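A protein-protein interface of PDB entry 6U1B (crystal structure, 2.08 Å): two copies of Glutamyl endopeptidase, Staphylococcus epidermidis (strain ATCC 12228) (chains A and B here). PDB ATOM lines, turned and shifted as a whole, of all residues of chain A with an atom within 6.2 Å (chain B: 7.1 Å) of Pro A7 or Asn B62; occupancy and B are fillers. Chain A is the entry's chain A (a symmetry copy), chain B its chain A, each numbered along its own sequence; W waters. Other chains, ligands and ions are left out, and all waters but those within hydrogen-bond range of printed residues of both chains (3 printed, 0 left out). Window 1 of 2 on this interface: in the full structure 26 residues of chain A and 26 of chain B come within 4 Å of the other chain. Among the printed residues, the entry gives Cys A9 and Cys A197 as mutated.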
ATOM      1  N   SER A   5       6.762  -7.950 -22.015  1.00  0.00           N
ATOM      2  CA  SER A   5       7.988  -7.164 -22.023  1.00  0.00           C
ATOM      3  C   SER A   5       7.691  -5.802 -22.637  1.00  0.00           C
ATOM      4  O   SER A   5       6.678  -5.613 -23.313  1.00  0.00           O
ATOM      5  CB  SER A   5       9.115  -7.874 -22.790  1.00  0.00           C
ATOM      6  OG  SER A   5       8.848  -7.903 -24.180  1.00  0.00           O
ATOM      7  N   TYR A   6       8.584  -4.849 -22.376  1.00  0.00           N
ATOM      8  CA  TYR A   6       8.488  -3.504 -22.950  1.00  0.00           C
ATOM      9  C   TYR A   6       9.906  -3.033 -23.244  1.00  0.00           C
ATOM     10  O   TYR A   6      10.476  -2.210 -22.516  1.00  0.00           O
ATOM     11  CB  TYR A   6       7.747  -2.559 -22.001  1.00  0.00           C
ATOM     12  CG  TYR A   6       7.218  -1.291 -22.645  1.00  0.00           C
ATOM     13  CD1 TYR A   6       6.138  -1.332 -23.522  1.00  0.00           C
ATOM     14  CD2 TYR A   6       7.791  -0.054 -22.364  1.00  0.00           C
ATOM     15  CE1 TYR A   6       5.647  -0.167 -24.108  1.00  0.00           C
ATOM     16  CE2 TYR A   6       7.312   1.114 -22.945  1.00  0.00           C
ATOM     17  CZ  TYR A   6       6.236   1.054 -23.812  1.00  0.00           C
ATOM     18  OH  TYR A   6       5.759   2.216 -24.387  1.00  0.00           O
ATOM     19  N   PRO A   7      10.523  -3.569 -24.300  1.00  0.00           N
ATOM     20  CA  PRO A   7      11.948  -3.278 -24.540  1.00  0.00           C
ATOM     21  C   PRO A   7      12.229  -1.842 -24.949  1.00  0.00           C
ATOM     22  O   PRO A   7      13.354  -1.375 -24.730  1.00  0.00           O
ATOM     23  CB  PRO A   7      12.325  -4.252 -25.664  1.00  0.00           C
ATOM     24  CG  PRO A   7      11.033  -4.461 -26.408  1.00  0.00           C
ATOM     25  CD  PRO A   7       9.962  -4.478 -25.316  1.00  0.00           C
ATOM     26  N   SER A   8      11.276  -1.117 -25.535  1.00  0.00           N
ATOM     27  CA  SER A   8      11.597   0.234 -25.971  1.00  0.00           C
ATOM     28  C   SER A   8      10.368   1.129 -25.852  1.00  0.00           C
ATOM     29  O   SER A   8       9.255   0.678 -25.563  1.00  0.00           O
ATOM     30  CB  SER A   8      12.183   0.234 -27.382  1.00  0.00           C
ATOM     31  OG  SER A   8      11.196  -0.043 -28.340  1.00  0.00           O
ATOM     32  N   CYS A   9      10.590   2.419 -26.072  1.00  0.00           N
ATOM     33  CA  CYS A   9       9.767   3.448 -25.456  1.00  0.00           C
ATOM     34  C   CYS A   9       9.138   4.382 -26.475  1.00  0.00           C
ATOM     35  O   CYS A   9       9.793   4.807 -27.436  1.00  0.00           O
ATOM     36  CB  CYS A   9      10.608   4.272 -24.491  1.00  0.00           C
ATOM     37  SG  CYS A   9      11.720   3.262 -23.473  1.00  0.00           S
ATOM     38  N   HIS A  59      19.096 -10.735 -28.281  1.00  0.00           N
ATOM     39  CA  HIS A  59      17.868 -11.138 -27.590  1.00  0.00           C
ATOM     40  C   HIS A  59      16.752 -11.479 -28.568  1.00  0.00           C
ATOM     41  O   HIS A  59      15.786 -12.144 -28.175  1.00  0.00           O
ATOM     42  CB  HIS A  59      17.410 -10.065 -26.567  1.00  0.00           C
ATOM     43  CG  HIS A  59      16.684  -8.890 -27.166  1.00  0.00           C
ATOM     44  ND1 HIS A  59      17.292  -7.672 -27.386  1.00  0.00           N
ATOM     45  CD2 HIS A  59      15.396  -8.740 -27.566  1.00  0.00           C
ATOM     46  CE1 HIS A  59      16.416  -6.825 -27.903  1.00  0.00           C
ATOM     47  NE2 HIS A  59      15.258  -7.448 -28.025  1.00  0.00           N
ATOM     48  N   VAL A 173       8.912   0.697 -30.622  1.00  0.00           N
ATOM     49  CA  VAL A 173       7.985  -0.186 -29.910  1.00  0.00           C
ATOM     50  C   VAL A 173       8.485  -1.616 -30.061  1.00  0.00           C
ATOM     51  O   VAL A 173       8.991  -1.988 -31.126  1.00  0.00           O
ATOM     52  CB  VAL A 173       6.540  -0.077 -30.466  1.00  0.00           C
ATOM     53  CG1 VAL A 173       5.623  -1.033 -29.748  1.00  0.00           C
ATOM     54  CG2 VAL A 173       5.999   1.347 -30.355  1.00  0.00           C
ATOM     55  N   GLY A 174       8.333  -2.415 -29.003  1.00  0.00           N
ATOM     56  CA  GLY A 174       8.570  -3.847 -29.069  1.00  0.00           C
ATOM     57  C   GLY A 174       8.200  -4.433 -30.419  1.00  0.00           C
ATOM     58  O   GLY A 174       7.076  -4.238 -30.904  1.00  0.00           O
ATOM     59  N   GLY A 175       9.148  -5.137 -31.048  1.00  0.00           N
ATOM     60  CA  GLY A 175       9.106  -5.460 -32.459  1.00  0.00           C
ATOM     61  C   GLY A 175      10.194  -4.747 -33.255  1.00  0.00           C
ATOM     62  O   GLY A 175      10.717  -5.313 -34.230  1.00  0.00           O
ATOM     63  N   SER A 177      13.135  -4.293 -32.198  1.00  0.00           N
ATOM     64  CA  SER A 177      14.420  -4.902 -31.846  1.00  0.00           C
ATOM     65  C   SER A 177      15.170  -5.400 -33.079  1.00  0.00           C
ATOM     66  O   SER A 177      14.647  -6.215 -33.848  1.00  0.00           O
ATOM     67  CB  SER A 177      14.208  -6.066 -30.879  1.00  0.00           C
ATOM     68  OG  SER A 177      13.773  -5.607 -29.613  1.00  0.00           O
ATOM     69  N   HIS A 192      19.219  -0.923 -33.563  1.00  0.00           N
ATOM     70  CA  HIS A 192      18.362  -0.674 -32.407  1.00  0.00           C
ATOM     71  C   HIS A 192      18.220  -1.931 -31.535  1.00  0.00           C
ATOM     72  O   HIS A 192      18.058  -3.046 -32.037  1.00  0.00           O
ATOM     73  CB  HIS A 192      16.987  -0.181 -32.897  1.00  0.00           C
ATOM     74  CG  HIS A 192      15.947  -0.117 -31.823  1.00  0.00           C
ATOM     75  ND1 HIS A 192      15.836   0.950 -30.960  1.00  0.00           N
ATOM     76  CD2 HIS A 192      14.985  -1.000 -31.462  1.00  0.00           C
ATOM     77  CE1 HIS A 192      14.841   0.728 -30.118  1.00  0.00           C
ATOM     78  NE2 HIS A 192      14.309  -0.449 -30.400  1.00  0.00           N
ATOM     79  N   TYR A 193      18.299  -1.757 -30.214  1.00  0.00           N
ATOM     80  CA  TYR A 193      18.067  -2.870 -29.293  1.00  0.00           C
ATOM     81  C   TYR A 193      17.122  -2.562 -28.135  1.00  0.00           C
ATOM     82  O   TYR A 193      16.609  -3.503 -27.530  1.00  0.00           O
ATOM     83  CB  TYR A 193      19.398  -3.390 -28.707  1.00  0.00           C
ATOM     84  CG  TYR A 193      19.995  -2.516 -27.614  1.00  0.00           C
ATOM     85  CD1 TYR A 193      19.572  -2.639 -26.284  1.00  0.00           C
ATOM     86  CD2 TYR A 193      20.999  -1.576 -27.906  1.00  0.00           C
ATOM     87  CE1 TYR A 193      20.100  -1.831 -25.286  1.00  0.00           C
ATOM     88  CE2 TYR A 193      21.547  -0.776 -26.909  1.00  0.00           C
ATOM     89  CZ  TYR A 193      21.086  -0.913 -25.599  1.00  0.00           C
ATOM     90  OH  TYR A 193      21.593  -0.127 -24.589  1.00  0.00           O
ATOM     91  N   GLY A 194      16.916  -1.303 -27.764  1.00  0.00           N
ATOM     92  CA  GLY A 194      16.120  -1.012 -26.578  1.00  0.00           C
ATOM     93  C   GLY A 194      16.012   0.461 -26.222  1.00  0.00           C
ATOM     94  O   GLY A 194      15.940   1.313 -27.109  1.00  0.00           O
ATOM     95  N   GLY A 195      16.002   0.765 -24.928  1.00  0.00           N
ATOM     96  CA  GLY A 195      15.881   2.136 -24.475  1.00  0.00           C
ATOM     97  C   GLY A 195      15.695   2.189 -22.977  1.00  0.00           C
ATOM     98  O   GLY A 195      15.690   1.167 -22.293  1.00  0.00           O
ATOM     99  N   VAL A 196      15.552   3.415 -22.479  1.00  0.00           N
ATOM    100  CA  VAL A 196      15.248   3.689 -21.074  1.00  0.00           C
ATOM    101  C   VAL A 196      14.013   4.581 -21.058  1.00  0.00           C
ATOM    102  O   VAL A 196      14.070   5.735 -21.500  1.00  0.00           O
ATOM    103  CB  VAL A 196      16.421   4.358 -20.343  1.00  0.00           C
ATOM    104  CG1 VAL A 196      15.972   4.883 -18.982  1.00  0.00           C
ATOM    105  CG2 VAL A 196      17.585   3.366 -20.175  1.00  0.00           C
ATOM    106  N   CYS A 197      12.891   4.048 -20.586  1.00  0.00           N
ATOM    107  CA  CYS A 197      11.633   4.781 -20.698  1.00  0.00           C
ATOM    108  C   CYS A 197      11.481   5.793 -19.545  1.00  0.00           C
ATOM    109  O   CYS A 197      11.802   5.476 -18.404  1.00  0.00           O
ATOM    110  CB  CYS A 197      10.450   3.809 -20.712  1.00  0.00           C
ATOM    111  SG  CYS A 197      10.520   2.511 -22.002  1.00  0.00           S
ATOM    112  N   ASN A 198      11.032   7.015 -19.833  1.00  0.00           N
ATOM    113  CA  ASN A 198      10.863   7.528 -21.184  1.00  0.00           C
ATOM    114  C   ASN A 198      11.920   8.597 -21.452  1.00  0.00           C
ATOM    115  O   ASN A 198      11.591   9.770 -21.631  1.00  0.00           O
ATOM    116  CB  ASN A 198       9.462   8.123 -21.372  1.00  0.00           C
ATOM    117  CG  ASN A 198       8.379   7.078 -21.385  1.00  0.00           C
ATOM    118  OD1 ASN A 198       8.513   6.032 -22.026  1.00  0.00           O
ATOM    119  ND2 ASN A 198       7.278   7.358 -20.685  1.00  0.00           N
ATOM    120  N   ASN A 201      15.846   6.012 -26.547  1.00  0.00           N
ATOM    121  CA  ASN A 201      15.982   4.662 -27.065  1.00  0.00           C
ATOM    122  C   ASN A 201      17.425   4.463 -27.511  1.00  0.00           C
ATOM    123  O   ASN A 201      18.167   5.432 -27.717  1.00  0.00           O
ATOM    124  CB  ASN A 201      14.964   4.403 -28.192  1.00  0.00           C
ATOM    125  CG  ASN A 201      13.555   4.215 -27.649  1.00  0.00           C
ATOM    126  OD1 ASN A 201      13.364   3.508 -26.656  1.00  0.00           O
ATOM    127  ND2 ASN A 201      12.573   4.876 -28.260  1.00  0.00           N
ATOM    128  N   ILE B  35       4.804  -5.822 -12.371  1.00  0.00           N
ATOM    129  CA  ILE B  35       4.439  -4.604 -13.077  1.00  0.00           C
ATOM    130  C   ILE B  35       3.201  -4.884 -13.927  1.00  0.00           C
ATOM    131  O   ILE B  35       3.267  -5.691 -14.864  1.00  0.00           O
ATOM    132  CB  ILE B  35       5.578  -4.072 -13.963  1.00  0.00           C
ATOM    133  CG1 ILE B  35       6.848  -3.808 -13.148  1.00  0.00           C
ATOM    134  CG2 ILE B  35       5.124  -2.801 -14.687  1.00  0.00           C
ATOM    135  CD1 ILE B  35       8.080  -3.431 -13.999  1.00  0.00           C
ATOM    136  N   ILE B  37       0.846  -4.304 -16.952  1.00  0.00           N
ATOM    137  CA  ILE B  37       1.051  -3.694 -18.260  1.00  0.00           C
ATOM    138  C   ILE B  37       0.106  -4.356 -19.255  1.00  0.00           C
ATOM    139  O   ILE B  37      -0.055  -5.580 -19.253  1.00  0.00           O
ATOM    140  CB  ILE B  37       2.529  -3.807 -18.702  1.00  0.00           C
ATOM    141  CG1 ILE B  37       2.729  -3.196 -20.099  1.00  0.00           C
ATOM    142  CG2 ILE B  37       3.014  -5.263 -18.612  1.00  0.00           C
ATOM    143  CD1 ILE B  37       4.195  -3.076 -20.526  1.00  0.00           C
ATOM    144  N   MET B  42       4.038  -7.978 -16.247  1.00  0.00           N
ATOM    145  CA  MET B  42       5.435  -8.330 -16.423  1.00  0.00           C
ATOM    146  C   MET B  42       6.001  -8.618 -15.038  1.00  0.00           C
ATOM    147  O   MET B  42       5.585  -7.995 -14.058  1.00  0.00           O
ATOM    148  CB  MET B  42       6.201  -7.169 -17.084  1.00  0.00           C
ATOM    149  CG  MET B  42       7.716  -7.362 -17.222  1.00  0.00           C
ATOM    150  SD  MET B  42       8.535  -5.851 -17.830  1.00  0.00           S
ATOM    151  CE  MET B  42       7.290  -5.314 -18.987  1.00  0.00           C
ATOM    152  N   ASN B  57      17.245  -4.548 -13.894  1.00  0.00           N
ATOM    153  CA  ASN B  57      17.630  -4.179 -15.256  1.00  0.00           C
ATOM    154  C   ASN B  57      16.902  -2.921 -15.708  1.00  0.00           C
ATOM    155  O   ASN B  57      15.782  -2.649 -15.275  1.00  0.00           O
ATOM    156  CB  ASN B  57      17.334  -5.297 -16.259  1.00  0.00           C
ATOM    157  CG  ASN B  57      18.107  -6.582 -15.977  1.00  0.00           C
ATOM    158  OD1 ASN B  57      17.612  -7.676 -16.264  1.00  0.00           O
ATOM    159  ND2 ASN B  57      19.320  -6.457 -15.416  1.00  0.00           N
ATOM    160  N   LYS B  58      17.557  -2.153 -16.591  1.00  0.00           N
ATOM    161  CA  LYS B  58      16.850  -1.122 -17.353  1.00  0.00           C
ATOM    162  C   LYS B  58      15.609  -1.692 -18.042  1.00  0.00           C
ATOM    163  O   LYS B  58      14.528  -1.084 -18.011  1.00  0.00           O
ATOM    164  CB  LYS B  58      17.774  -0.492 -18.404  1.00  0.00           C
ATOM    165  CG  LYS B  58      18.746   0.567 -17.889  1.00  0.00           C
ATOM    166  CD  LYS B  58      19.853   0.782 -18.913  1.00  0.00           C
ATOM    167  CE  LYS B  58      20.793   1.895 -18.511  1.00  0.00           C
ATOM    168  NZ  LYS B  58      22.059   1.830 -19.293  1.00  0.00           N
ATOM    169  N   HIS B  59      15.741  -2.856 -18.688  1.00  0.00           N
ATOM    170  CA  HIS B  59      14.602  -3.365 -19.458  1.00  0.00           C
ATOM    171  C   HIS B  59      13.492  -3.881 -18.554  1.00  0.00           C
ATOM    172  O   HIS B  59      12.354  -4.026 -19.017  1.00  0.00           O
ATOM    173  CB  HIS B  59      15.043  -4.444 -20.482  1.00  0.00           C
ATOM    174  CG  HIS B  59      15.259  -5.816 -19.899  1.00  0.00           C
ATOM    175  ND1 HIS B  59      16.511  -6.317 -19.618  1.00  0.00           N
ATOM    176  CD2 HIS B  59      14.383  -6.799 -19.572  1.00  0.00           C
ATOM    177  CE1 HIS B  59      16.401  -7.544 -19.133  1.00  0.00           C
ATOM    178  NE2 HIS B  59      15.119  -7.861 -19.093  1.00  0.00           N
ATOM    179  N   VAL B  60      13.776  -4.114 -17.271  1.00  0.00           N
ATOM    180  CA  VAL B  60      12.716  -4.470 -16.327  1.00  0.00           C
ATOM    181  C   VAL B  60      11.910  -3.239 -15.931  1.00  0.00           C
ATOM    182  O   VAL B  60      10.683  -3.222 -16.068  1.00  0.00           O
ATOM    183  CB  VAL B  60      13.285  -5.182 -15.081  1.00  0.00           C
ATOM    184  CG1 VAL B  60      12.233  -5.220 -13.973  1.00  0.00           C
ATOM    185  CG2 VAL B  60      13.711  -6.596 -15.413  1.00  0.00           C
ATOM    186  N   VAL B  61      12.573  -2.202 -15.407  1.00  0.00           N
ATOM    187  CA  VAL B  61      11.827  -1.014 -14.984  1.00  0.00           C
ATOM    188  C   VAL B  61      11.085  -0.366 -16.150  1.00  0.00           C
ATOM    189  O   VAL B  61      10.086   0.321 -15.930  1.00  0.00           O
ATOM    190  CB  VAL B  61      12.742   0.014 -14.284  1.00  0.00           C
ATOM    191  CG1 VAL B  61      13.272  -0.559 -12.973  1.00  0.00           C
ATOM    192  CG2 VAL B  61      13.887   0.436 -15.192  1.00  0.00           C
ATOM    193  N   ASN B  62      11.549  -0.588 -17.389  1.00  0.00           N
ATOM    194  CA  ASN B  62      10.881  -0.057 -18.579  1.00  0.00           C
ATOM    195  C   ASN B  62       9.417  -0.443 -18.633  1.00  0.00           C
ATOM    196  O   ASN B  62       8.611   0.276 -19.232  1.00  0.00           O
ATOM    197  CB  ASN B  62      11.556  -0.566 -19.858  1.00  0.00           C
ATOM    198  CG  ASN B  62      12.748   0.266 -20.267  1.00  0.00           C
ATOM    199  OD1 ASN B  62      13.057   1.289 -19.653  1.00  0.00           O
ATOM    200  ND2 ASN B  62      13.441  -0.183 -21.303  1.00  0.00           N
ATOM    201  N   GLY B  63       9.056  -1.580 -18.028  1.00  0.00           N
ATOM    202  CA  GLY B  63       7.675  -2.019 -18.048  1.00  0.00           C
ATOM    203  C   GLY B  63       6.717  -1.034 -17.427  1.00  0.00           C
ATOM    204  O   GLY B  63       5.524  -1.079 -17.724  1.00  0.00           O
ATOM    205  N   ALA B  64       7.213  -0.153 -16.563  1.00  0.00           N
ATOM    206  CA  ALA B  64       6.411   0.884 -15.930  1.00  0.00           C
ATOM    207  C   ALA B  64       6.109   2.048 -16.864  1.00  0.00           C
ATOM    208  O   ALA B  64       5.374   2.958 -16.463  1.00  0.00           O
ATOM    209  CB  ALA B  64       7.122   1.418 -14.683  1.00  0.00           C
ATOM    210  N   LYS B  65       6.678   2.053 -18.068  1.00  0.00           N
ATOM    211  CA  LYS B  65       6.448   3.114 -19.053  1.00  0.00           C
ATOM    212  C   LYS B  65       6.723   4.499 -18.463  1.00  0.00           C
ATOM    213  O   LYS B  65       5.968   5.450 -18.670  1.00  0.00           O
ATOM    214  CB  LYS B  65       5.030   3.025 -19.624  1.00  0.00           C
ATOM    215  CG  LYS B  65       4.739   1.697 -20.325  1.00  0.00           C
ATOM    216  CD  LYS B  65       3.474   1.764 -21.173  1.00  0.00           C
ATOM    217  CE  LYS B  65       3.107   0.394 -21.733  1.00  0.00           C
ATOM    218  NZ  LYS B  65       1.860   0.429 -22.542  1.00  0.00           N
ATOM    219  N   GLY B  66       7.816   4.610 -17.704  1.00  0.00           N
ATOM    220  CA  GLY B  66       8.275   5.878 -17.182  1.00  0.00           C
ATOM    221  C   GLY B  66       7.746   6.240 -15.812  1.00  0.00           C
ATOM    222  O   GLY B  66       8.265   7.181 -15.196  1.00  0.00           O
ATOM    223  N   ASN B  67       6.737   5.530 -15.307  1.00  0.00           N
ATOM    224  CA  ASN B  67       6.115   5.858 -14.022  1.00  0.00           C
ATOM    225  C   ASN B  67       6.509   4.852 -12.941  1.00  0.00           C
ATOM    226  O   ASN B  67       5.918   3.763 -12.873  1.00  0.00           O
ATOM    227  CB  ASN B  67       4.592   5.889 -14.186  1.00  0.00           C
ATOM    228  CG  ASN B  67       3.859   6.133 -12.866  1.00  0.00           C
ATOM    229  OD1 ASN B  67       4.472   6.355 -11.818  1.00  0.00           O
ATOM    230  ND2 ASN B  67       2.534   6.119 -12.927  1.00  0.00           N
ATOM    231  N   ILE B  71       5.436  -0.030 -10.377  1.00  0.00           N
ATOM    232  CA  ILE B  71       6.287  -1.161 -10.016  1.00  0.00           C
ATOM    233  C   ILE B  71       6.029  -1.564  -8.569  1.00  0.00           C
ATOM    234  O   ILE B  71       6.080  -0.726  -7.665  1.00  0.00           O
ATOM    235  CB  ILE B  71       7.774  -0.824 -10.217  1.00  0.00           C
ATOM    236  CG1 ILE B  71       8.032  -0.319 -11.635  1.00  0.00           C
ATOM    237  CG2 ILE B  71       8.636  -2.050  -9.898  1.00  0.00           C
ATOM    238  CD1 ILE B  71       9.434   0.255 -11.844  1.00  0.00           C
ATOM    239  N   ILE B  93      13.250   6.027 -10.739  1.00  0.00           N
ATOM    240  CA  ILE B  93      14.073   5.147 -11.558  1.00  0.00           C
ATOM    241  C   ILE B  93      15.369   5.875 -11.893  1.00  0.00           C
ATOM    242  O   ILE B  93      15.349   6.968 -12.470  1.00  0.00           O
ATOM    243  CB  ILE B  93      13.332   4.721 -12.838  1.00  0.00           C
ATOM    244  CG1 ILE B  93      12.140   3.816 -12.488  1.00  0.00           C
ATOM    245  CG2 ILE B  93      14.312   4.068 -13.824  1.00  0.00           C
ATOM    246  CD1 ILE B  93      11.185   3.563 -13.658  1.00  0.00           C
ATOM    247  N   ASP B 101      22.805  -2.880 -18.937  1.00  0.00           N
ATOM    248  CA  ASP B 101      21.383  -3.064 -18.637  1.00  0.00           C
ATOM    249  C   ASP B 101      21.176  -3.086 -17.113  1.00  0.00           C
ATOM    250  O   ASP B 101      20.801  -4.092 -16.506  1.00  0.00           O
ATOM    251  CB  ASP B 101      20.891  -4.351 -19.306  1.00  0.00           C
ATOM    252  CG  ASP B 101      19.361  -4.470 -19.353  1.00  0.00           C
ATOM    253  OD1 ASP B 101      18.646  -3.621 -18.757  1.00  0.00           O
ATOM    254  OD2 ASP B 101      18.865  -5.441 -19.975  1.00  0.00           O
HETATM  255  O   HOH W   1      12.562   3.136 -17.370  1.00  0.00           O
HETATM  256  O   HOH W   2      11.026  -5.362 -20.919  1.00  0.00           O
HETATM  257  O   HOH W   3      22.070  -1.206 -21.895  1.00  0.00           O
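The side-chain amide oxygen of Asn B62 sits at hydrogen-bond distance from the backbone NH of Cys A197 (2.9 Å).
The backbone carbonyl oxygen (O) of Gly A195 is in hydrogen-bond range of the side-chain amide nitrogen (ND2) of Asn B62, 2.8 Å away.
The side-chain amide nitrogen of Asn A198 is in hydrogen-bond range of the backbone carbonyl oxygen of Lys B65 (3.1 Å).
OD1 of Asp B101 is in hydrogen-bond range of N of Lys B58 (2.8 Å).
The side-chain sulfur (SG) of Cys A197 is disulfide-bonded to the side-chain sulfur (SG) of Cys A9, 2.0 Å away.
The backbone carbonyl oxygen (O) of Lys B58 lies close to the side-chain amide oxygen (OD1) of Asn B62, 3.2 Å away.
The backbone NH (N) of Met B42 lies within hydrogen-bond range of the backbone carbonyl oxygen (O) of Ile B35.
The backbone carbonyl oxygen (O) of Pro A7 sits at hydrogen-bond distance from the backbone NH (N) of Gly A195, at 3.4 Å.
Among the printed residues, merely in contact across the chains: Ser A5 with Met B42 (3.6 Å), Tyr A6 with Ile B37 (3.9 Å), Tyr A6 with Met B42 (3.7 Å), Tyr A6 with Asn B62 (3.3 Å), Tyr A6 with Gly B63 (3.99 Å), Tyr A6 with Lys B65 (3.5 Å), Pro A7 with Asn B62 (3.6 Å), Val A196 with Lys B58 (3.7 Å), Val A196 with Asn B62 (3.5 Å), Cys A197 with Gly B66 (3.8 Å) and Asn A198 with Gly B66 (3.9 Å).
Of the printed residues of chain B, Pro A7 touches Asn B62 (3.6 Å).
Printed residues of chain A within 4 Å of Asn B62: Tyr A6 (3.3 Å), Pro A7 (3.6 Å), Gly A195 (2.8 Å), Val A196 (3.5 Å) and Cys A197 (2.9 Å).
Of the printed residues of chain B, Ser A5 touches Met B42 (3.6 Å).
Of the printed residues of chain A, Ile B37 touches Tyr A6.
Printed residues of chain A within 4 Å of Met B42: Ser A5 (3.6 Å) and Tyr A6 (3.7 Å).
Of the printed residues of chain B, Cys A197 touches Asn B62 and Gly B66.
The nearest residue of chain A that does not touch Asn B62 is Cys A9 (4.4 Å).
Of the 17 printed residues of chain B, 7 touch a printed residue of chain A.
Printed residues of chain A that touch a printed residue of chain B: Ser A5, Tyr A6, Pro A7, Gly A195, Val A196, Cys A197 and Asn A198.
Hydrophobic or aromatic side chains of chain A within 4 Å of the printed part of chain B: Tyr A6 and Val A196.
Among the printed residues, 14 pairs touch across the chains.
Among the printed residues, no Asp or Glu carboxylate lies within 4 Å of a Lys or Arg side-chain nitrogen of the other chain.
Position printed for both chains: 59.
Of the 14 pairs that touch across the chains among the printed residues, none has its exchanged pair printed and touching as well.
Water W1 lies within hydrogen-bond range of O of Cys A197 (2.7 Å) and OD1 of Asn B62 (3.0 Å).
Water W2 lies within hydrogen-bond range of the backbone carbonyl oxygen (O) of His B59 and the backbone NH (N) of Tyr A6.
Water W3 bridges the side-chain hydroxyl (OH) of Tyr A193 (2.9 Å) and the backbone NH (N) of Asp B101 (3.5 Å).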
